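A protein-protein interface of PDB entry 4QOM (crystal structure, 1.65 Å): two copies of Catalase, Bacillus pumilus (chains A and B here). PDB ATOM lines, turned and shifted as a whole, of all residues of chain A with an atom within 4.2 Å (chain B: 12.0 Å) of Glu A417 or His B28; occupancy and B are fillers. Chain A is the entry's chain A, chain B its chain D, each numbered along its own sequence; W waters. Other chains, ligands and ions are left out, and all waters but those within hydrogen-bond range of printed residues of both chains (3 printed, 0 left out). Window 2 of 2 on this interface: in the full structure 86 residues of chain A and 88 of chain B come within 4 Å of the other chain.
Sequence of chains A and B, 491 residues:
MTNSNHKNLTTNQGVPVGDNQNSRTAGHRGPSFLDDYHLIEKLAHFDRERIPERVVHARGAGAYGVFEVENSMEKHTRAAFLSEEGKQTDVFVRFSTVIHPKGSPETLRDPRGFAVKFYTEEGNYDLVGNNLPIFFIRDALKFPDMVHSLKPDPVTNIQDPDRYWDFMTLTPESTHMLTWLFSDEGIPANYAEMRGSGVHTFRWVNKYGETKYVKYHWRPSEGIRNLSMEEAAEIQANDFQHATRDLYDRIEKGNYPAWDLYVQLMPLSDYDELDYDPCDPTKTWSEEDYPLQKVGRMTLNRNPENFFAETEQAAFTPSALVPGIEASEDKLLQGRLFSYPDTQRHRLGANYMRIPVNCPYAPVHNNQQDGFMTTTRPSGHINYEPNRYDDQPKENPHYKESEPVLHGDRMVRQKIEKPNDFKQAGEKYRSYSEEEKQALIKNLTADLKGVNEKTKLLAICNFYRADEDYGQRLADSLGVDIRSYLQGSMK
O of His B28 is in hydrogen-bond range of NZ of Lys A331. The side-chain carboxylate of Glu A417 lies close to a ring nitrogen (ND1) of His B28 (3.4 Å). N of Lys A415 is in hydrogen-bond range of OD1 of Asn B22.
The side-chain hydroxyl of Thr B25 lies within hydrogen-bond range of the backbone carbonyl oxygen of Gly B27 (2.5 Å). The side-chain carboxylate of Asp B19 sits at hydrogen-bond distance from the side-chain amide nitrogen of Asn B22. The backbone carbonyl oxygen (O) of Gln A414 is in hydrogen-bond range of the side-chain amino group (NZ) of Lys A331 (2.7 Å).
Among the printed residues, merely in contact across the chains: Ile A416 with His B28, Gln A414 with His B28, Gln A414 with Asn B22, Lys A415 with His B28 and Lys A331 with Thr B25.
Printed residues of chain A within 4 Å of His B28: Lys A331, Gln A414, Lys A415, Ile A416 and Glu A417. Gln A414 touches just these residues of chain B: Asn B22 (3.6 Å) and His B28 (3.6 Å). No residue of chain B comes within 4 Å of Lys A418. No residue of chain B comes within 4 Å of Pro A419. Of the printed residues of chain B, Lys A331 touches Thr B25 and His B28. Of the printed residues of chain A, Thr B25 touches Lys A331 (3.9 Å). Of the printed residues of chain A, Asn B22 touches Gln A414 (3.6 Å) and Lys A415 (3.4 Å). Of the printed residues of chain B, Lys A415 touches Asn B22 and His B28. Ser B23 touches none of the printed residues of chain A. Gly B30 touches none of the printed residues of chain A. The nearest residue of chain B that does not touch Glu A417 is Arg B29 (5.6 Å). The nearest printed residue of chain A that does not touch Asn B22 is Lys A331 (5.0 Å).
Of the 15 printed residues of chain B, 3 touch a printed residue of chain A. Hydrophobic or aromatic side chains of chain B within 4 Å of the printed part of chain A: His B28. Printed residues of chain A that touch a printed residue of chain B: Lys A331, Gln A414, Lys A415, Ile A416 and Glu A417. Hydrophobic or aromatic side chains of chain A within 4 Å of the printed part of chain B: Ile A416. Among the printed residues, no Asp or Glu carboxylate lies within 4 Å of a Lys or Arg side-chain nitrogen of the other chain.
No position is printed for both chains.
Water W1 lies within hydrogen-bond range of the side-chain hydroxyl of Thr B25 (2.6 Å), the backbone carbonyl oxygen of Ser B23 (2.7 Å), the side-chain amino group of Lys A331 (2.9 Å) and the backbone NH of Gln A414 (3.1 Å). Water W3 bridges OD1 of Asn B22 (2.7 Å) and NZ of Lys A331 (3.1 Å). Water W2 lies within hydrogen-bond range of OG of Ser B32 (2.8 Å), O of Lys A331 (2.9 Å) and OG of Ser B23 (2.9 Å).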
ATOM      1  N   LYS A 331       4.250  28.256  -7.374  1.00  0.00           N
ATOM      2  CA  LYS A 331       3.541  27.037  -7.115  1.00  0.00           C
ATOM      3  C   LYS A 331       2.911  26.539  -8.446  1.00  0.00           C
ATOM      4  O   LYS A 331       2.533  25.372  -8.534  1.00  0.00           O
ATOM      5  CB  LYS A 331       2.429  27.225  -6.107  1.00  0.00           C
ATOM      6  CG  LYS A 331       2.938  27.594  -4.703  1.00  0.00           C
ATOM      7  CD  LYS A 331       1.792  27.648  -3.712  1.00  0.00           C
ATOM      8  CE  LYS A 331       2.208  28.355  -2.422  1.00  0.00           C
ATOM      9  NZ  LYS A 331       1.029  28.354  -1.511  1.00  0.00           N
ATOM     10  N   GLN A 414      -1.730  26.513   1.886  1.00  0.00           N
ATOM     11  CA  GLN A 414      -2.097  27.878   2.213  1.00  0.00           C
ATOM     12  C   GLN A 414      -1.694  28.851   1.110  1.00  0.00           C
ATOM     13  O   GLN A 414      -0.593  28.764   0.591  1.00  0.00           O
ATOM     14  CB  GLN A 414      -1.355  28.216   3.498  1.00  0.00           C
ATOM     15  CG  GLN A 414      -1.717  29.498   4.210  1.00  0.00           C
ATOM     16  CD  GLN A 414      -0.766  29.694   5.377  1.00  0.00           C
ATOM     17  OE1 GLN A 414      -0.279  28.712   5.965  1.00  0.00           O
ATOM     18  NE2 GLN A 414      -0.432  30.946   5.678  1.00  0.00           N
ATOM     19  N   LYS A 415      -2.555  29.813   0.836  1.00  0.00           N
ATOM     20  CA  LYS A 415      -2.290  30.784  -0.177  1.00  0.00           C
ATOM     21  C   LYS A 415      -1.071  31.579   0.189  1.00  0.00           C
ATOM     22  O   LYS A 415      -0.819  31.853   1.380  1.00  0.00           O
ATOM     23  CB  LYS A 415      -3.482  31.730  -0.340  1.00  0.00           C
ATOM     24  CG  LYS A 415      -3.363  32.674  -1.523  1.00  0.00           C
ATOM     25  CD  LYS A 415      -4.436  33.748  -1.464  1.00  0.00           C
ATOM     26  CE  LYS A 415      -5.821  33.188  -1.696  1.00  0.00           C
ATOM     27  NZ  LYS A 415      -6.709  34.368  -1.849  1.00  0.00           N
ATOM     28  N   ILE A 416      -0.315  31.987  -0.816  1.00  0.00           N
ATOM     29  CA  ILE A 416       0.792  32.921  -0.558  1.00  0.00           C
ATOM     30  C   ILE A 416       0.335  34.179   0.178  1.00  0.00           C
ATOM     31  O   ILE A 416      -0.844  34.644   0.052  1.00  0.00           O
ATOM     32  CB  ILE A 416       1.465  33.405  -1.864  1.00  0.00           C
ATOM     33  CG1 ILE A 416       0.479  34.062  -2.789  1.00  0.00           C
ATOM     34  CG2 ILE A 416       2.235  32.268  -2.538  1.00  0.00           C
ATOM     35  CD1 ILE A 416       1.125  34.824  -3.900  1.00  0.00           C
ATOM     36  N   GLU A 417       1.282  34.768   0.940  1.00  0.00           N
ATOM     37  CA  GLU A 417       1.095  36.125   1.436  1.00  0.00           C
ATOM     38  C   GLU A 417       1.195  37.147   0.319  1.00  0.00           C
ATOM     39  O   GLU A 417       1.689  36.883  -0.772  1.00  0.00           O
ATOM     40  CB  GLU A 417       2.096  36.396   2.575  1.00  0.00           C
ATOM     41  CG  GLU A 417       2.118  35.254   3.596  1.00  0.00           C
ATOM     42  CD  GLU A 417       1.815  35.607   5.040  1.00  0.00           C
ATOM     43  OE1 GLU A 417       2.443  34.996   5.924  1.00  0.00           O
ATOM     44  OE2 GLU A 417       0.889  36.396   5.299  1.00  0.00           O
ATOM     45  N   LYS A 418       0.701  38.342   0.601  1.00  0.00           N
ATOM     46  CA  LYS A 418       0.592  39.458  -0.378  1.00  0.00           C
ATOM     47  C   LYS A 418       0.044  39.055  -1.767  1.00  0.00           C
ATOM     48  O   LYS A 418       0.644  39.429  -2.762  1.00  0.00           O
ATOM     49  CB  LYS A 418       1.965  40.099  -0.591  1.00  0.00           C
ATOM     50  CG  LYS A 418       2.801  40.428   0.675  1.00  0.00           C
ATOM     51  CD  LYS A 418       4.193  41.010   0.252  1.00  0.00           C
ATOM     52  CE  LYS A 418       5.315  39.990  -0.052  1.00  0.00           C
ATOM     53  NZ  LYS A 418       6.566  40.716  -0.422  1.00  0.00           N
ATOM     54  N   PRO A 419      -1.143  38.448  -1.806  1.00  0.00           N
ATOM     55  CA  PRO A 419      -1.691  38.103  -3.127  1.00  0.00           C
ATOM     56  C   PRO A 419      -1.954  39.349  -3.995  1.00  0.00           C
ATOM     57  O   PRO A 419      -1.743  39.291  -5.198  1.00  0.00           O
ATOM     58  CB  PRO A 419      -3.008  37.360  -2.796  1.00  0.00           C
ATOM     59  CG  PRO A 419      -3.318  37.785  -1.375  1.00  0.00           C
ATOM     60  CD  PRO A 419      -1.986  37.944  -0.701  1.00  0.00           C
ATOM     61  N   ASP B  19      -9.009  20.562   0.719  1.00  0.00           N
ATOM     62  CA  ASP B  19      -8.538  21.816   0.113  1.00  0.00           C
ATOM     63  C   ASP B  19      -8.308  21.554  -1.348  1.00  0.00           C
ATOM     64  O   ASP B  19      -7.362  20.838  -1.729  1.00  0.00           O
ATOM     65  CB  ASP B  19      -7.217  22.320   0.789  1.00  0.00           C
ATOM     66  CG  ASP B  19      -6.799  23.768   0.354  1.00  0.00           C
ATOM     67  OD1 ASP B  19      -7.262  24.262  -0.721  1.00  0.00           O
ATOM     68  OD2 ASP B  19      -6.005  24.404   1.101  1.00  0.00           O
ATOM     69  N   GLN B  21      -7.881  24.154  -3.415  1.00  0.00           N
ATOM     70  CA  GLN B  21      -7.264  25.380  -3.903  1.00  0.00           C
ATOM     71  C   GLN B  21      -5.732  25.382  -3.862  1.00  0.00           C
ATOM     72  O   GLN B  21      -5.116  25.963  -4.749  1.00  0.00           O
ATOM     73  CB  GLN B  21      -7.799  26.595  -3.122  1.00  0.00           C
ATOM     74  CG  GLN B  21      -9.283  26.575  -2.832  1.00  0.00           C
ATOM     75  CD  GLN B  21     -10.150  26.175  -4.001  1.00  0.00           C
ATOM     76  OE1 GLN B  21      -9.990  26.676  -5.140  1.00  0.00           O
ATOM     77  NE2 GLN B  21     -11.114  25.300  -3.737  1.00  0.00           N
ATOM     78  N   ASN B  22      -5.118  24.842  -2.796  1.00  0.00           N
ATOM     79  CA  ASN B  22      -3.703  24.984  -2.561  1.00  0.00           C
ATOM     80  C   ASN B  22      -2.991  23.686  -2.654  1.00  0.00           C
ATOM     81  O   ASN B  22      -3.386  22.716  -1.972  1.00  0.00           O
ATOM     82  CB  ASN B  22      -3.461  25.622  -1.157  1.00  0.00           C
ATOM     83  CG  ASN B  22      -4.169  26.940  -0.986  1.00  0.00           C
ATOM     84  OD1 ASN B  22      -3.903  27.912  -1.706  1.00  0.00           O
ATOM     85  ND2 ASN B  22      -5.226  26.912  -0.191  1.00  0.00           N
ATOM     86  N   SER B  23      -1.898  23.708  -3.395  1.00  0.00           N
ATOM     87  CA  SER B  23      -0.880  22.645  -3.375  1.00  0.00           C
ATOM     88  C   SER B  23      -0.245  22.543  -1.988  1.00  0.00           C
ATOM     89  O   SER B  23      -0.244  23.523  -1.189  1.00  0.00           O
ATOM     90  CB  SER B  23       0.179  22.888  -4.434  1.00  0.00           C
ATOM     91  OG  SER B  23      -0.361  22.688  -5.718  1.00  0.00           O
ATOM     92  N   ARG B  24       0.368  21.385  -1.669  1.00  0.00           N
ATOM     93  CA  ARG B  24       1.063  21.236  -0.388  1.00  0.00           C
ATOM     94  C   ARG B  24       2.535  21.661  -0.521  1.00  0.00           C
ATOM     95  O   ARG B  24       3.273  21.145  -1.384  1.00  0.00           O
ATOM     96  CB  ARG B  24       0.962  19.785   0.047  1.00  0.00           C
ATOM     97  CG  ARG B  24       1.207  19.560   1.481  1.00  0.00           C
ATOM     98  CD  ARG B  24       0.956  18.094   1.732  1.00  0.00           C
ATOM     99  NE  ARG B  24       0.785  17.871   3.129  1.00  0.00           N
ATOM    100  CZ  ARG B  24       0.875  16.701   3.719  1.00  0.00           C
ATOM    101  NH1 ARG B  24       1.215  15.632   3.026  1.00  0.00           N
ATOM    102  NH2 ARG B  24       0.726  16.652   5.059  1.00  0.00           N
ATOM    103  N   THR B  25       2.964  22.595   0.325  1.00  0.00           N
ATOM    104  CA  THR B  25       4.195  23.291   0.087  1.00  0.00           C
ATOM    105  C   THR B  25       4.934  23.549   1.390  1.00  0.00           C
ATOM    106  O   THR B  25       4.404  23.342   2.486  1.00  0.00           O
ATOM    107  CB  THR B  25       3.911  24.665  -0.604  1.00  0.00           C
ATOM    108  OG1 THR B  25       3.101  25.492   0.249  1.00  0.00           O
ATOM    109  CG2 THR B  25       3.298  24.516  -1.954  1.00  0.00           C
ATOM    110  N   ALA B  26       6.206  23.861   1.263  1.00  0.00           N
ATOM    111  CA  ALA B  26       7.037  24.196   2.424  1.00  0.00           C
ATOM    112  C   ALA B  26       6.765  25.625   2.894  1.00  0.00           C
ATOM    113  O   ALA B  26       7.415  26.567   2.454  1.00  0.00           O
ATOM    114  CB  ALA B  26       8.524  23.960   2.123  1.00  0.00           C
ATOM    115  N   GLY B  27       5.800  25.750   3.786  1.00  0.00           N
ATOM    116  CA  GLY B  27       5.224  27.024   4.126  1.00  0.00           C
ATOM    117  C   GLY B  27       4.382  27.623   2.997  1.00  0.00           C
ATOM    118  O   GLY B  27       4.213  27.035   1.928  1.00  0.00           O
ATOM    119  N   HIS B  28       3.878  28.823   3.226  1.00  0.00           N
ATOM    120  CA  HIS B  28       2.935  29.395   2.334  1.00  0.00           C
ATOM    121  C   HIS B  28       3.527  29.783   0.975  1.00  0.00           C
ATOM    122  O   HIS B  28       2.759  29.975   0.043  1.00  0.00           O
ATOM    123  CB  HIS B  28       2.217  30.602   2.974  1.00  0.00           C
ATOM    124  CG  HIS B  28       3.142  31.696   3.381  1.00  0.00           C
ATOM    125  ND1 HIS B  28       3.415  31.978   4.701  1.00  0.00           N
ATOM    126  CD2 HIS B  28       3.907  32.536   2.643  1.00  0.00           C
ATOM    127  CE1 HIS B  28       4.292  32.962   4.756  1.00  0.00           C
ATOM    128  NE2 HIS B  28       4.622  33.302   3.522  1.00  0.00           N
ATOM    129  N   ARG B  29       4.843  29.956   0.870  1.00  0.00           N
ATOM    130  CA  ARG B  29       5.412  30.357  -0.412  1.00  0.00           C
ATOM    131  C   ARG B  29       6.522  29.440  -0.928  1.00  0.00           C
ATOM    132  O   ARG B  29       7.276  29.789  -1.854  1.00  0.00           O
ATOM    133  CB  ARG B  29       5.839  31.828  -0.437  1.00  0.00           C
ATOM    134  CG  ARG B  29       6.975  32.226   0.492  1.00  0.00           C
ATOM    135  CD  ARG B  29       7.244  33.733   0.302  1.00  0.00           C
ATOM    136  NE  ARG B  29       8.546  34.157   0.844  1.00  0.00           N
ATOM    137  CZ  ARG B  29       9.714  33.996   0.221  1.00  0.00           C
ATOM    138  NH1 ARG B  29       9.761  33.387  -0.968  1.00  0.00           N
ATOM    139  NH2 ARG B  29      10.828  34.455   0.790  1.00  0.00           N
ATOM    140  N   GLY B  30       6.637  28.264  -0.354  1.00  0.00           N
ATOM    141  CA  GLY B  30       7.852  27.458  -0.598  1.00  0.00           C
ATOM    142  C   GLY B  30       7.505  26.510  -1.728  1.00  0.00           C
ATOM    143  O   GLY B  30       6.379  26.503  -2.230  1.00  0.00           O
ATOM    144  N   PRO B  31       8.479  25.686  -2.089  1.00  0.00           N
ATOM    145  CA  PRO B  31       8.273  24.706  -3.157  1.00  0.00           C
ATOM    146  C   PRO B  31       7.336  23.601  -2.717  1.00  0.00           C
ATOM    147  O   PRO B  31       7.030  23.438  -1.539  1.00  0.00           O
ATOM    148  CB  PRO B  31       9.703  24.189  -3.420  1.00  0.00           C
ATOM    149  CG  PRO B  31      10.427  24.448  -2.204  1.00  0.00           C
ATOM    150  CD  PRO B  31       9.877  25.720  -1.681  1.00  0.00           C
ATOM    151  N   SER B  32       6.924  22.792  -3.691  1.00  0.00           N
ATOM    152  CA  SER B  32       5.863  21.805  -3.531  1.00  0.00           C
ATOM    153  C   SER B  32       6.400  20.425  -3.157  1.00  0.00           C
ATOM    154  O   SER B  32       7.452  20.015  -3.626  1.00  0.00           O
ATOM    155  CB  SER B  32       5.059  21.717  -4.808  1.00  0.00           C
ATOM    156  OG  SER B  32       4.340  22.964  -5.103  1.00  0.00           O
ATOM    157  N   PHE B  33       5.630  19.718  -2.357  1.00  0.00           N
ATOM    158  CA  PHE B  33       5.960  18.436  -1.897  1.00  0.00           C
ATOM    159  C   PHE B  33       5.390  17.348  -2.830  1.00  0.00           C
ATOM    160  O   PHE B  33       4.275  17.487  -3.384  1.00  0.00           O
ATOM    161  CB  PHE B  33       5.432  18.241  -0.508  1.00  0.00           C
ATOM    162  CG  PHE B  33       6.296  18.917   0.504  1.00  0.00           C
ATOM    163  CD1 PHE B  33       7.627  18.547   0.641  1.00  0.00           C
ATOM    164  CD2 PHE B  33       5.830  19.995   1.256  1.00  0.00           C
ATOM    165  CE1 PHE B  33       8.460  19.145   1.540  1.00  0.00           C
ATOM    166  CE2 PHE B  33       6.685  20.643   2.136  1.00  0.00           C
ATOM    167  CZ  PHE B  33       8.021  20.228   2.246  1.00  0.00           C
ATOM    168  N   ASP B  36       1.470  14.829  -2.163  1.00  0.00           N
ATOM    169  CA  ASP B  36       0.219  15.561  -2.378  1.00  0.00           C
ATOM    170  C   ASP B  36      -0.625  14.717  -3.373  1.00  0.00           C
ATOM    171  O   ASP B  36      -0.588  14.941  -4.583  1.00  0.00           O
ATOM    172  CB  ASP B  36       0.493  16.949  -2.938  1.00  0.00           C
ATOM    173  CG  ASP B  36      -0.758  17.814  -2.934  1.00  0.00           C
ATOM    174  OD1 ASP B  36      -1.870  17.247  -2.834  1.00  0.00           O
ATOM    175  OD2 ASP B  36      -0.623  19.047  -3.117  1.00  0.00           O
HETATM  176  O   HOH W   1       0.513  25.903  -0.126  1.00  0.00           O
HETATM  177  O   HOH W   2       2.275  22.991  -6.942  1.00  0.00           O
HETATM  178  O   HOH W   3      -1.612  28.167  -3.087  1.00  0.00           O
